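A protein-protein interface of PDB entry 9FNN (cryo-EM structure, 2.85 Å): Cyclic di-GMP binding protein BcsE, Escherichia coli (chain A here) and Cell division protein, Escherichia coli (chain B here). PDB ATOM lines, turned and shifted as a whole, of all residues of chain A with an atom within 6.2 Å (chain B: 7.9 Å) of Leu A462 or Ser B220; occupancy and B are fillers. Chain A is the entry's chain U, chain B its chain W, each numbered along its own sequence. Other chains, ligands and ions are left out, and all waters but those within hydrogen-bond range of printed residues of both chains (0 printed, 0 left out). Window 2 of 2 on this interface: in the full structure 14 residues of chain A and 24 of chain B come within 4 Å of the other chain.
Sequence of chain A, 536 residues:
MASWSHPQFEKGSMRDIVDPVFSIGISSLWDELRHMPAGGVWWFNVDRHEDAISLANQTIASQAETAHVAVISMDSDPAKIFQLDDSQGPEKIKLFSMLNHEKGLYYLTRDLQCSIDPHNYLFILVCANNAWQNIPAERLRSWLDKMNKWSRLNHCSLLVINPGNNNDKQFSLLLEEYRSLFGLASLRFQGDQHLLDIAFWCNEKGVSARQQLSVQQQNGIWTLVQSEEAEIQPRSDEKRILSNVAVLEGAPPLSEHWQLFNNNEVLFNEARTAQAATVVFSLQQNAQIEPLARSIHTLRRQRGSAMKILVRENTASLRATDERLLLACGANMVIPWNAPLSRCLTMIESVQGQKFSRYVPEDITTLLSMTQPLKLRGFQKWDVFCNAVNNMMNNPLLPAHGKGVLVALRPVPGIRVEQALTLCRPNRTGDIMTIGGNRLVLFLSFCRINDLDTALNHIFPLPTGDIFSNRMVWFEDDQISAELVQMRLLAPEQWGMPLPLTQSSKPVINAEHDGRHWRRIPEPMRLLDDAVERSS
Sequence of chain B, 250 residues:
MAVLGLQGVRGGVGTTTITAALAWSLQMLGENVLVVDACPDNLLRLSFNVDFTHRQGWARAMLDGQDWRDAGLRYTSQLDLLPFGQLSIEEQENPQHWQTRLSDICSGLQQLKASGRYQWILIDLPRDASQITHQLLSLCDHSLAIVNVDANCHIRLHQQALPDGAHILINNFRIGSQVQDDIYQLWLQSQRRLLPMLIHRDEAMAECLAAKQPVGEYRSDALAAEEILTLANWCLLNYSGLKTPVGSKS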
ATOM      1  N   LEU A 456      -4.378  29.625 -25.506  1.00  0.00           N
ATOM      2  CA  LEU A 456      -4.961  28.447 -24.875  1.00  0.00           C
ATOM      3  C   LEU A 456      -4.607  28.389 -23.396  1.00  0.00           C
ATOM      4  O   LEU A 456      -5.448  28.036 -22.562  1.00  0.00           O
ATOM      5  CB  LEU A 456      -4.505  27.180 -25.593  1.00  0.00           C
ATOM      6  CG  LEU A 456      -5.010  27.006 -27.024  1.00  0.00           C
ATOM      7  CD1 LEU A 456      -4.588  25.663 -27.581  1.00  0.00           C
ATOM      8  CD2 LEU A 456      -6.514  27.151 -27.073  1.00  0.00           C
ATOM      9  N   ASN A 457      -3.366  28.733 -23.052  1.00  0.00           N
ATOM     10  CA  ASN A 457      -2.959  28.776 -21.656  1.00  0.00           C
ATOM     11  C   ASN A 457      -3.711  29.851 -20.886  1.00  0.00           C
ATOM     12  O   ASN A 457      -3.936  29.705 -19.680  1.00  0.00           O
ATOM     13  CB  ASN A 457      -1.455  29.011 -21.565  1.00  0.00           C
ATOM     14  CG  ASN A 457      -0.649  27.852 -22.112  1.00  0.00           C
ATOM     15  OD1 ASN A 457      -1.119  26.718 -22.153  1.00  0.00           O
ATOM     16  ND2 ASN A 457       0.575  28.132 -22.530  1.00  0.00           N
ATOM     17  N   HIS A 458      -4.102  30.932 -21.556  1.00  0.00           N
ATOM     18  CA  HIS A 458      -4.876  31.972 -20.890  1.00  0.00           C
ATOM     19  C   HIS A 458      -6.334  31.581 -20.692  1.00  0.00           C
ATOM     20  O   HIS A 458      -6.964  32.040 -19.734  1.00  0.00           O
ATOM     21  CB  HIS A 458      -4.801  33.277 -21.679  1.00  0.00           C
ATOM     22  CG  HIS A 458      -3.486  33.980 -21.565  1.00  0.00           C
ATOM     23  ND1 HIS A 458      -3.188  35.121 -22.274  1.00  0.00           N
ATOM     24  CD2 HIS A 458      -2.390  33.703 -20.820  1.00  0.00           C
ATOM     25  CE1 HIS A 458      -1.966  35.518 -21.972  1.00  0.00           C
ATOM     26  NE2 HIS A 458      -1.460  34.675 -21.092  1.00  0.00           N
ATOM     27  N   PHE A 460      -7.593  28.390 -20.393  1.00  0.00           N
ATOM     28  CA  PHE A 460      -7.734  26.993 -19.908  1.00  0.00           C
ATOM     29  C   PHE A 460      -6.804  26.785 -18.719  1.00  0.00           C
ATOM     30  O   PHE A 460      -5.834  27.561 -18.594  1.00  0.00           O
ATOM     31  CB  PHE A 460      -7.293  25.993 -20.979  1.00  0.00           C
ATOM     32  CG  PHE A 460      -8.283  25.727 -22.083  1.00  0.00           C
ATOM     33  CD1 PHE A 460      -9.501  25.127 -21.815  1.00  0.00           C
ATOM     34  CD2 PHE A 460      -7.989  26.067 -23.393  1.00  0.00           C
ATOM     35  CE1 PHE A 460     -10.405  24.877 -22.835  1.00  0.00           C
ATOM     36  CE2 PHE A 460      -8.895  25.821 -24.411  1.00  0.00           C
ATOM     37  CZ  PHE A 460     -10.104  25.229 -24.129  1.00  0.00           C
ATOM     38  N   PRO A 461      -7.045  25.800 -17.823  1.00  0.00           N
ATOM     39  CA  PRO A 461      -6.084  25.491 -16.766  1.00  0.00           C
ATOM     40  C   PRO A 461      -4.738  25.374 -17.491  1.00  0.00           C
ATOM     41  O   PRO A 461      -4.657  24.562 -18.402  1.00  0.00           O
ATOM     42  CB  PRO A 461      -6.557  24.154 -16.179  1.00  0.00           C
ATOM     43  CG  PRO A 461      -7.727  23.722 -17.050  1.00  0.00           C
ATOM     44  CD  PRO A 461      -8.242  24.969 -17.737  1.00  0.00           C
ATOM     45  N   LEU A 462      -3.736  26.168 -17.096  1.00  0.00           N
ATOM     46  CA  LEU A 462      -2.426  26.207 -17.817  1.00  0.00           C
ATOM     47  C   LEU A 462      -2.067  24.861 -18.474  1.00  0.00           C
ATOM     48  O   LEU A 462      -1.831  24.887 -19.697  1.00  0.00           O
ATOM     49  CB  LEU A 462      -1.325  26.699 -16.870  1.00  0.00           C
ATOM     50  CG  LEU A 462      -0.646  27.994 -17.312  1.00  0.00           C
ATOM     51  CD1 LEU A 462      -1.118  29.169 -16.471  1.00  0.00           C
ATOM     52  CD2 LEU A 462       0.868  27.865 -17.260  1.00  0.00           C
ATOM     53  N   PRO A 463      -1.981  23.703 -17.772  1.00  0.00           N
ATOM     54  CA  PRO A 463      -1.562  22.448 -18.417  1.00  0.00           C
ATOM     55  C   PRO A 463      -2.528  21.943 -19.502  1.00  0.00           C
ATOM     56  O   PRO A 463      -3.390  21.141 -19.179  1.00  0.00           O
ATOM     57  CB  PRO A 463      -1.519  21.418 -17.275  1.00  0.00           C
ATOM     58  CG  PRO A 463      -1.461  22.243 -16.016  1.00  0.00           C
ATOM     59  CD  PRO A 463      -2.233  23.503 -16.339  1.00  0.00           C
ATOM     60  N   THR A 464      -2.378  22.418 -20.745  1.00  0.00           N
ATOM     61  CA  THR A 464      -3.199  21.876 -21.865  1.00  0.00           C
ATOM     62  C   THR A 464      -2.674  20.467 -22.142  1.00  0.00           C
ATOM     63  O   THR A 464      -1.438  20.292 -22.101  1.00  0.00           O
ATOM     64  CB  THR A 464      -3.154  22.798 -23.092  1.00  0.00           C
ATOM     65  OG1 THR A 464      -3.167  24.156 -22.650  1.00  0.00           O
ATOM     66  CG2 THR A 464      -4.309  22.568 -24.042  1.00  0.00           C
ATOM     67  N   TRP A 518      -6.970  30.848 -13.629  1.00  0.00           N
ATOM     68  CA  TRP A 518      -7.191  29.458 -13.257  1.00  0.00           C
ATOM     69  C   TRP A 518      -6.145  29.044 -12.232  1.00  0.00           C
ATOM     70  O   TRP A 518      -4.942  29.168 -12.483  1.00  0.00           O
ATOM     71  CB  TRP A 518      -7.114  28.545 -14.477  1.00  0.00           C
ATOM     72  CG  TRP A 518      -8.391  28.406 -15.228  1.00  0.00           C
ATOM     73  CD1 TRP A 518      -8.685  28.933 -16.448  1.00  0.00           C
ATOM     74  CD2 TRP A 518      -9.548  27.678 -14.815  1.00  0.00           C
ATOM     75  NE1 TRP A 518      -9.957  28.581 -16.820  1.00  0.00           N
ATOM     76  CE2 TRP A 518     -10.508  27.809 -15.832  1.00  0.00           C
ATOM     77  CE3 TRP A 518      -9.868  26.928 -13.682  1.00  0.00           C
ATOM     78  CZ2 TRP A 518     -11.763  27.222 -15.751  1.00  0.00           C
ATOM     79  CZ3 TRP A 518     -11.114  26.346 -13.605  1.00  0.00           C
ATOM     80  CH2 TRP A 518     -12.045  26.497 -14.631  1.00  0.00           C
ATOM     81  N   ARG A 520      -5.154  25.660  -9.878  1.00  0.00           N
ATOM     82  CA  ARG A 520      -5.420  24.250  -9.643  1.00  0.00           C
ATOM     83  C   ARG A 520      -5.361  23.941  -8.156  1.00  0.00           C
ATOM     84  O   ARG A 520      -4.386  24.277  -7.478  1.00  0.00           O
ATOM     85  CB  ARG A 520      -4.428  23.383 -10.407  1.00  0.00           C
ATOM     86  CG  ARG A 520      -4.810  23.173 -11.847  1.00  0.00           C
ATOM     87  CD  ARG A 520      -3.926  22.144 -12.488  1.00  0.00           C
ATOM     88  NE  ARG A 520      -4.472  21.680 -13.754  1.00  0.00           N
ATOM     89  CZ  ARG A 520      -5.165  20.562 -13.900  1.00  0.00           C
ATOM     90  NH1 ARG A 520      -5.419  19.768 -12.874  1.00  0.00           N
ATOM     91  NH2 ARG A 520      -5.612  20.229 -15.108  1.00  0.00           N
ATOM     92  N   TRP B  24       7.420  21.929 -12.289  1.00  0.00           N
ATOM     93  CA  TRP B  24       6.428  22.409 -13.245  1.00  0.00           C
ATOM     94  C   TRP B  24       6.938  22.304 -14.675  1.00  0.00           C
ATOM     95  O   TRP B  24       6.206  21.883 -15.576  1.00  0.00           O
ATOM     96  CB  TRP B  24       6.042  23.849 -12.922  1.00  0.00           C
ATOM     97  CG  TRP B  24       4.997  24.386 -13.826  1.00  0.00           C
ATOM     98  CD1 TRP B  24       5.180  25.217 -14.886  1.00  0.00           C
ATOM     99  CD2 TRP B  24       3.595  24.121 -13.761  1.00  0.00           C
ATOM    100  NE1 TRP B  24       3.978  25.491 -15.486  1.00  0.00           N
ATOM    101  CE2 TRP B  24       2.989  24.829 -14.811  1.00  0.00           C
ATOM    102  CE3 TRP B  24       2.794  23.354 -12.914  1.00  0.00           C
ATOM    103  CZ2 TRP B  24       1.619  24.792 -15.037  1.00  0.00           C
ATOM    104  CZ3 TRP B  24       1.438  23.319 -13.142  1.00  0.00           C
ATOM    105  CH2 TRP B  24       0.863  24.034 -14.192  1.00  0.00           C
ATOM    106  N   GLN B  27       7.076  18.609 -15.820  1.00  0.00           N
ATOM    107  CA  GLN B  27       5.751  18.101 -16.156  1.00  0.00           C
ATOM    108  C   GLN B  27       5.171  18.786 -17.386  1.00  0.00           C
ATOM    109  O   GLN B  27       4.305  18.206 -18.049  1.00  0.00           O
ATOM    110  CB  GLN B  27       4.803  18.240 -14.963  1.00  0.00           C
ATOM    111  CG  GLN B  27       4.322  19.644 -14.680  1.00  0.00           C
ATOM    112  CD  GLN B  27       2.947  19.906 -15.236  1.00  0.00           C
ATOM    113  OE1 GLN B  27       2.226  18.980 -15.596  1.00  0.00           O
ATOM    114  NE2 GLN B  27       2.573  21.174 -15.313  1.00  0.00           N
ATOM    115  N   MET B  28       5.623  20.000 -17.707  1.00  0.00           N
ATOM    116  CA  MET B  28       5.251  20.614 -18.974  1.00  0.00           C
ATOM    117  C   MET B  28       5.957  19.962 -20.153  1.00  0.00           C
ATOM    118  O   MET B  28       5.440  20.009 -21.273  1.00  0.00           O
ATOM    119  CB  MET B  28       5.559  22.109 -18.950  1.00  0.00           C
ATOM    120  CG  MET B  28       4.467  22.966 -18.344  1.00  0.00           C
ATOM    121  SD  MET B  28       3.009  23.058 -19.392  1.00  0.00           S
ATOM    122  CE  MET B  28       2.074  24.335 -18.565  1.00  0.00           C
ATOM    123  N   THR B  76      -1.407  18.125 -10.858  1.00  0.00           N
ATOM    124  CA  THR B  76      -1.847  17.847 -12.216  1.00  0.00           C
ATOM    125  C   THR B  76      -1.762  16.343 -12.447  1.00  0.00           C
ATOM    126  O   THR B  76      -1.395  15.576 -11.553  1.00  0.00           O
ATOM    127  CB  THR B  76      -1.004  18.600 -13.252  1.00  0.00           C
ATOM    128  OG1 THR B  76       0.325  18.064 -13.271  1.00  0.00           O
ATOM    129  CG2 THR B  76      -0.939  20.073 -12.916  1.00  0.00           C
ATOM    130  N   ALA B 204       8.989  37.824 -10.808  1.00  0.00           N
ATOM    131  CA  ALA B 204       8.078  36.692 -10.915  1.00  0.00           C
ATOM    132  C   ALA B 204       8.378  35.644  -9.853  1.00  0.00           C
ATOM    133  O   ALA B 204       7.458  35.060  -9.271  1.00  0.00           O
ATOM    134  CB  ALA B 204       8.162  36.080 -12.310  1.00  0.00           C
ATOM    135  N   GLN B 213       1.645  29.682  -6.551  1.00  0.00           N
ATOM    136  CA  GLN B 213       1.785  28.988  -7.821  1.00  0.00           C
ATOM    137  C   GLN B 213       3.260  28.878  -8.172  1.00  0.00           C
ATOM    138  O   GLN B 213       4.065  29.711  -7.742  1.00  0.00           O
ATOM    139  CB  GLN B 213       1.049  29.726  -8.949  1.00  0.00           C
ATOM    140  CG  GLN B 213      -0.456  29.628  -8.885  1.00  0.00           C
ATOM    141  CD  GLN B 213      -1.132  30.417  -9.983  1.00  0.00           C
ATOM    142  OE1 GLN B 213      -2.171  30.013 -10.503  1.00  0.00           O
ATOM    143  NE2 GLN B 213      -0.552  31.553 -10.336  1.00  0.00           N
ATOM    144  N   PRO B 214       3.645  27.863  -8.942  1.00  0.00           N
ATOM    145  CA  PRO B 214       4.993  27.845  -9.515  1.00  0.00           C
ATOM    146  C   PRO B 214       5.160  28.963 -10.531  1.00  0.00           C
ATOM    147  O   PRO B 214       4.194  29.456 -11.116  1.00  0.00           O
ATOM    148  CB  PRO B 214       5.080  26.469 -10.181  1.00  0.00           C
ATOM    149  CG  PRO B 214       4.032  25.656  -9.516  1.00  0.00           C
ATOM    150  CD  PRO B 214       2.927  26.605  -9.195  1.00  0.00           C
ATOM    151  N   VAL B 215       6.416  29.370 -10.735  1.00  0.00           N
ATOM    152  CA  VAL B 215       6.674  30.531 -11.582  1.00  0.00           C
ATOM    153  C   VAL B 215       6.253  30.264 -13.019  1.00  0.00           C
ATOM    154  O   VAL B 215       5.809  31.179 -13.723  1.00  0.00           O
ATOM    155  CB  VAL B 215       8.153  30.960 -11.489  1.00  0.00           C
ATOM    156  CG1 VAL B 215       9.062  29.947 -12.146  1.00  0.00           C
ATOM    157  CG2 VAL B 215       8.344  32.330 -12.112  1.00  0.00           C
ATOM    158  N   GLY B 216       6.378  29.021 -13.482  1.00  0.00           N
ATOM    159  CA  GLY B 216       5.889  28.692 -14.809  1.00  0.00           C
ATOM    160  C   GLY B 216       4.387  28.843 -14.919  1.00  0.00           C
ATOM    161  O   GLY B 216       3.875  29.326 -15.932  1.00  0.00           O
ATOM    162  N   GLU B 217       3.659  28.431 -13.882  1.00  0.00           N
ATOM    163  CA  GLU B 217       2.214  28.626 -13.874  1.00  0.00           C
ATOM    164  C   GLU B 217       1.855  30.080 -13.611  1.00  0.00           C
ATOM    165  O   GLU B 217       0.921  30.614 -14.220  1.00  0.00           O
ATOM    166  CB  GLU B 217       1.566  27.711 -12.836  1.00  0.00           C
ATOM    167  CG  GLU B 217       0.098  27.997 -12.594  1.00  0.00           C
ATOM    168  CD  GLU B 217      -0.645  26.810 -12.029  1.00  0.00           C
ATOM    169  OE1 GLU B 217       0.012  25.827 -11.634  1.00  0.00           O
ATOM    170  OE2 GLU B 217      -1.890  26.856 -11.985  1.00  0.00           O
ATOM    171  N   TYR B 218       2.585  30.740 -12.713  1.00  0.00           N
ATOM    172  CA  TYR B 218       2.277  32.126 -12.382  1.00  0.00           C
ATOM    173  C   TYR B 218       2.505  33.043 -13.576  1.00  0.00           C
ATOM    174  O   TYR B 218       1.642  33.857 -13.918  1.00  0.00           O
ATOM    175  CB  TYR B 218       3.115  32.577 -11.188  1.00  0.00           C
ATOM    176  CG  TYR B 218       2.946  34.034 -10.842  1.00  0.00           C
ATOM    177  CD1 TYR B 218       1.788  34.491 -10.237  1.00  0.00           C
ATOM    178  CD2 TYR B 218       3.943  34.954 -11.120  1.00  0.00           C
ATOM    179  CE1 TYR B 218       1.626  35.819  -9.922  1.00  0.00           C
ATOM    180  CE2 TYR B 218       3.790  36.284 -10.806  1.00  0.00           C
ATOM    181  CZ  TYR B 218       2.629  36.711 -10.207  1.00  0.00           C
ATOM    182  OH  TYR B 218       2.470  38.039  -9.892  1.00  0.00           O
ATOM    183  N   ARG B 219       3.660  32.921 -14.227  1.00  0.00           N
ATOM    184  CA  ARG B 219       3.993  33.790 -15.353  1.00  0.00           C
ATOM    185  C   ARG B 219       4.964  33.028 -16.248  1.00  0.00           C
ATOM    186  O   ARG B 219       6.165  32.985 -15.967  1.00  0.00           O
ATOM    187  CB  ARG B 219       4.585  35.103 -14.865  1.00  0.00           C
ATOM    188  CG  ARG B 219       4.731  36.159 -15.940  1.00  0.00           C
ATOM    189  CD  ARG B 219       4.990  37.515 -15.317  1.00  0.00           C
ATOM    190  NE  ARG B 219       3.884  37.933 -14.468  1.00  0.00           N
ATOM    191  CZ  ARG B 219       3.946  38.925 -13.591  1.00  0.00           C
ATOM    192  NH1 ARG B 219       5.059  39.617 -13.409  1.00  0.00           N
ATOM    193  NH2 ARG B 219       2.868  39.228 -12.874  1.00  0.00           N
ATOM    194  N   SER B 220       4.440  32.434 -17.320  1.00  0.00           N
ATOM    195  CA  SER B 220       5.269  31.653 -18.226  1.00  0.00           C
ATOM    196  C   SER B 220       6.135  32.520 -19.126  1.00  0.00           C
ATOM    197  O   SER B 220       7.130  32.026 -19.666  1.00  0.00           O
ATOM    198  CB  SER B 220       4.391  30.742 -19.083  1.00  0.00           C
ATOM    199  OG  SER B 220       3.605  29.888 -18.270  1.00  0.00           O
ATOM    200  N   ASP B 221       5.785  33.792 -19.300  1.00  0.00           N
ATOM    201  CA  ASP B 221       6.562  34.687 -20.143  1.00  0.00           C
ATOM    202  C   ASP B 221       7.760  35.286 -19.420  1.00  0.00           C
ATOM    203  O   ASP B 221       8.599  35.923 -20.067  1.00  0.00           O
ATOM    204  CB  ASP B 221       5.666  35.809 -20.673  1.00  0.00           C
ATOM    205  CG  ASP B 221       6.226  36.469 -21.918  1.00  0.00           C
ATOM    206  OD1 ASP B 221       7.197  35.934 -22.494  1.00  0.00           O
ATOM    207  OD2 ASP B 221       5.696  37.526 -22.320  1.00  0.00           O
ATOM    208  N   ALA B 222       7.865  35.099 -18.110  1.00  0.00           N
ATOM    209  CA  ALA B 222       8.948  35.698 -17.351  1.00  0.00           C
ATOM    210  C   ALA B 222      10.273  35.018 -17.674  1.00  0.00           C
ATOM    211  O   ALA B 222      10.325  33.861 -18.099  1.00  0.00           O
ATOM    212  CB  ALA B 222       8.663  35.616 -15.854  1.00  0.00           C
ATOM    213  N   LEU B 223      11.358  35.765 -17.466  1.00  0.00           N
ATOM    214  CA  LEU B 223      12.682  35.270 -17.825  1.00  0.00           C
ATOM    215  C   LEU B 223      13.086  34.081 -16.963  1.00  0.00           C
ATOM    216  O   LEU B 223      13.728  33.143 -17.451  1.00  0.00           O
ATOM    217  CB  LEU B 223      13.705  36.398 -17.706  1.00  0.00           C
ATOM    218  CG  LEU B 223      15.115  36.109 -18.220  1.00  0.00           C
ATOM    219  CD1 LEU B 223      15.087  35.781 -19.703  1.00  0.00           C
ATOM    220  CD2 LEU B 223      16.032  37.287 -17.944  1.00  0.00           C
ATOM    221  N   ALA B 224      12.725  34.108 -15.679  1.00  0.00           N
ATOM    222  CA  ALA B 224      13.055  32.998 -14.794  1.00  0.00           C
ATOM    223  C   ALA B 224      12.364  31.716 -15.236  1.00  0.00           C
ATOM    224  O   ALA B 224      12.930  30.624 -15.116  1.00  0.00           O
ATOM    225  CB  ALA B 224      12.677  33.344 -13.358  1.00  0.00           C
ATOM    226  N   ALA B 225      11.139  31.827 -15.755  1.00  0.00           N
ATOM    227  CA  ALA B 225      10.451  30.654 -16.284  1.00  0.00           C
ATOM    228  C   ALA B 225      11.194  30.067 -17.476  1.00  0.00           C
ATOM    229  O   ALA B 225      11.338  28.843 -17.589  1.00  0.00           O
ATOM    230  CB  ALA B 225       9.020  31.017 -16.668  1.00  0.00           C
ATOM    231  N   GLU B 226      11.677  30.924 -18.377  1.00  0.00           N
ATOM    232  CA  GLU B 226      12.451  30.444 -19.516  1.00  0.00           C
ATOM    233  C   GLU B 226      13.749  29.784 -19.064  1.00  0.00           C
ATOM    234  O   GLU B 226      14.152  28.745 -19.606  1.00  0.00           O
ATOM    235  CB  GLU B 226      12.735  31.602 -20.472  1.00  0.00           C
ATOM    236  CG  GLU B 226      13.630  31.239 -21.646  1.00  0.00           C
ATOM    237  CD  GLU B 226      13.892  32.416 -22.565  1.00  0.00           C
ATOM    238  OE1 GLU B 226      13.184  33.438 -22.441  1.00  0.00           O
ATOM    239  OE2 GLU B 226      14.805  32.321 -23.412  1.00  0.00           O
ATOM    240  N   GLU B 227      14.415  30.366 -18.068  1.00  0.00           N
ATOM    241  CA  GLU B 227      15.644  29.770 -17.556  1.00  0.00           C
ATOM    242  C   GLU B 227      15.375  28.419 -16.903  1.00  0.00           C
ATOM    243  O   GLU B 227      16.168  27.480 -17.048  1.00  0.00           O
ATOM    244  CB  GLU B 227      16.316  30.728 -16.576  1.00  0.00           C
ATOM    245  CG  GLU B 227      16.912  31.953 -17.246  1.00  0.00           C
ATOM    246  CD  GLU B 227      17.158  33.091 -16.279  1.00  0.00           C
ATOM    247  OE1 GLU B 227      16.409  33.201 -15.286  1.00  0.00           O
ATOM    248  OE2 GLU B 227      18.099  33.877 -16.512  1.00  0.00           O
ATOM    249  N   LEU B 229      12.942  26.419 -17.734  1.00  0.00           N
ATOM    250  CA  LEU B 229      12.691  25.506 -18.844  1.00  0.00           C
ATOM    251  C   LEU B 229      13.997  25.020 -19.459  1.00  0.00           C
ATOM    252  O   LEU B 229      14.136  23.837 -19.798  1.00  0.00           O
ATOM    253  CB  LEU B 229      11.820  26.189 -19.894  1.00  0.00           C
ATOM    254  CG  LEU B 229      11.314  25.316 -21.037  1.00  0.00           C
ATOM    255  CD1 LEU B 229      10.440  24.201 -20.499  1.00  0.00           C
ATOM    256  CD2 LEU B 229      10.556  26.154 -22.050  1.00  0.00           C
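The side-chain hydroxyl (OG1) of Thr B76 lies within hydrogen-bond range of the side-chain amide oxygen (OE1) of Gln B27.
OE1 of Gln B213 lies close to OE2 of Glu B217 (3.5 Å).
The backbone carbonyl oxygen (O) of Gly B216 is in hydrogen-bond range of the side-chain hydroxyl (OG) of Ser B220.
The backbone carbonyl oxygen of Leu A462 is in hydrogen-bond range of the side-chain hydroxyl of Thr A464, 3.3 Å away.
The side-chain amide oxygen of Asn A457 sits close to the backbone carbonyl oxygen of Leu A462, 3.1 Å away.
Among the printed residues, pairs that only touch across the chains: Leu A462 with Trp B24 (3.9 Å), Leu A462 with Met B28 (3.95 Å), Leu A462 with Gly B216 (3.6 Å), Leu A462 with Glu B217 (3.4 Å), Leu A462 with Ser B220 (3.6 Å), Pro A463 with Trp B24 (3.5 Å), Pro A463 with Thr B76 (3.8 Å), Trp A518 with Gln B213 (3.5 Å), Trp A518 with Glu B217 (3.9 Å) and Arg A520 with Thr B76 (3.7 Å).
Leu A456 touches none of the printed residues of chain B.
Leu A462 touches five residues of chain B.
Printed residues of chain B within 4 Å of Pro A463: Trp B24 (3.5 Å) and Thr B76 (3.8 Å).
Thr A464 touches none of the printed residues of chain B.
Printed residues of chain B within 4 Å of Trp A518: Gln B213 and Glu B217.
Of the printed residues of chain A, Trp B24 touches Leu A462 and Pro A463.
Printed residues of chain A within 4 Å of Met B28: Leu A462 (3.95 Å).
Ser B220 touches just one residue of chain A: Leu A462 (3.6 Å).
The nearest residue of chain A that does not touch Ser B220 is Asn A457 (5.5 Å).
The nearest printed residue of chain A that does not touch Gln B213 is Arg A520 (5.3 Å).
Printed residues of chain A that touch a printed residue of chain B: Leu A462, Pro A463, Trp A518 and Arg A520.
Hydrophobic or aromatic side chains of chain A that line the printed part of chain B: Leu A462 and Pro A463.
Printed residues of chain B that touch a printed residue of chain A: Trp B24, Met B28, Thr B76, Gln B213, Gly B216, Glu B217 and Ser B220.
Hydrophobic or aromatic side chains of chain B that line the printed part of chain A: Trp B24 and Met B28.
Among the printed residues, 10 pairs touch across the chains.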
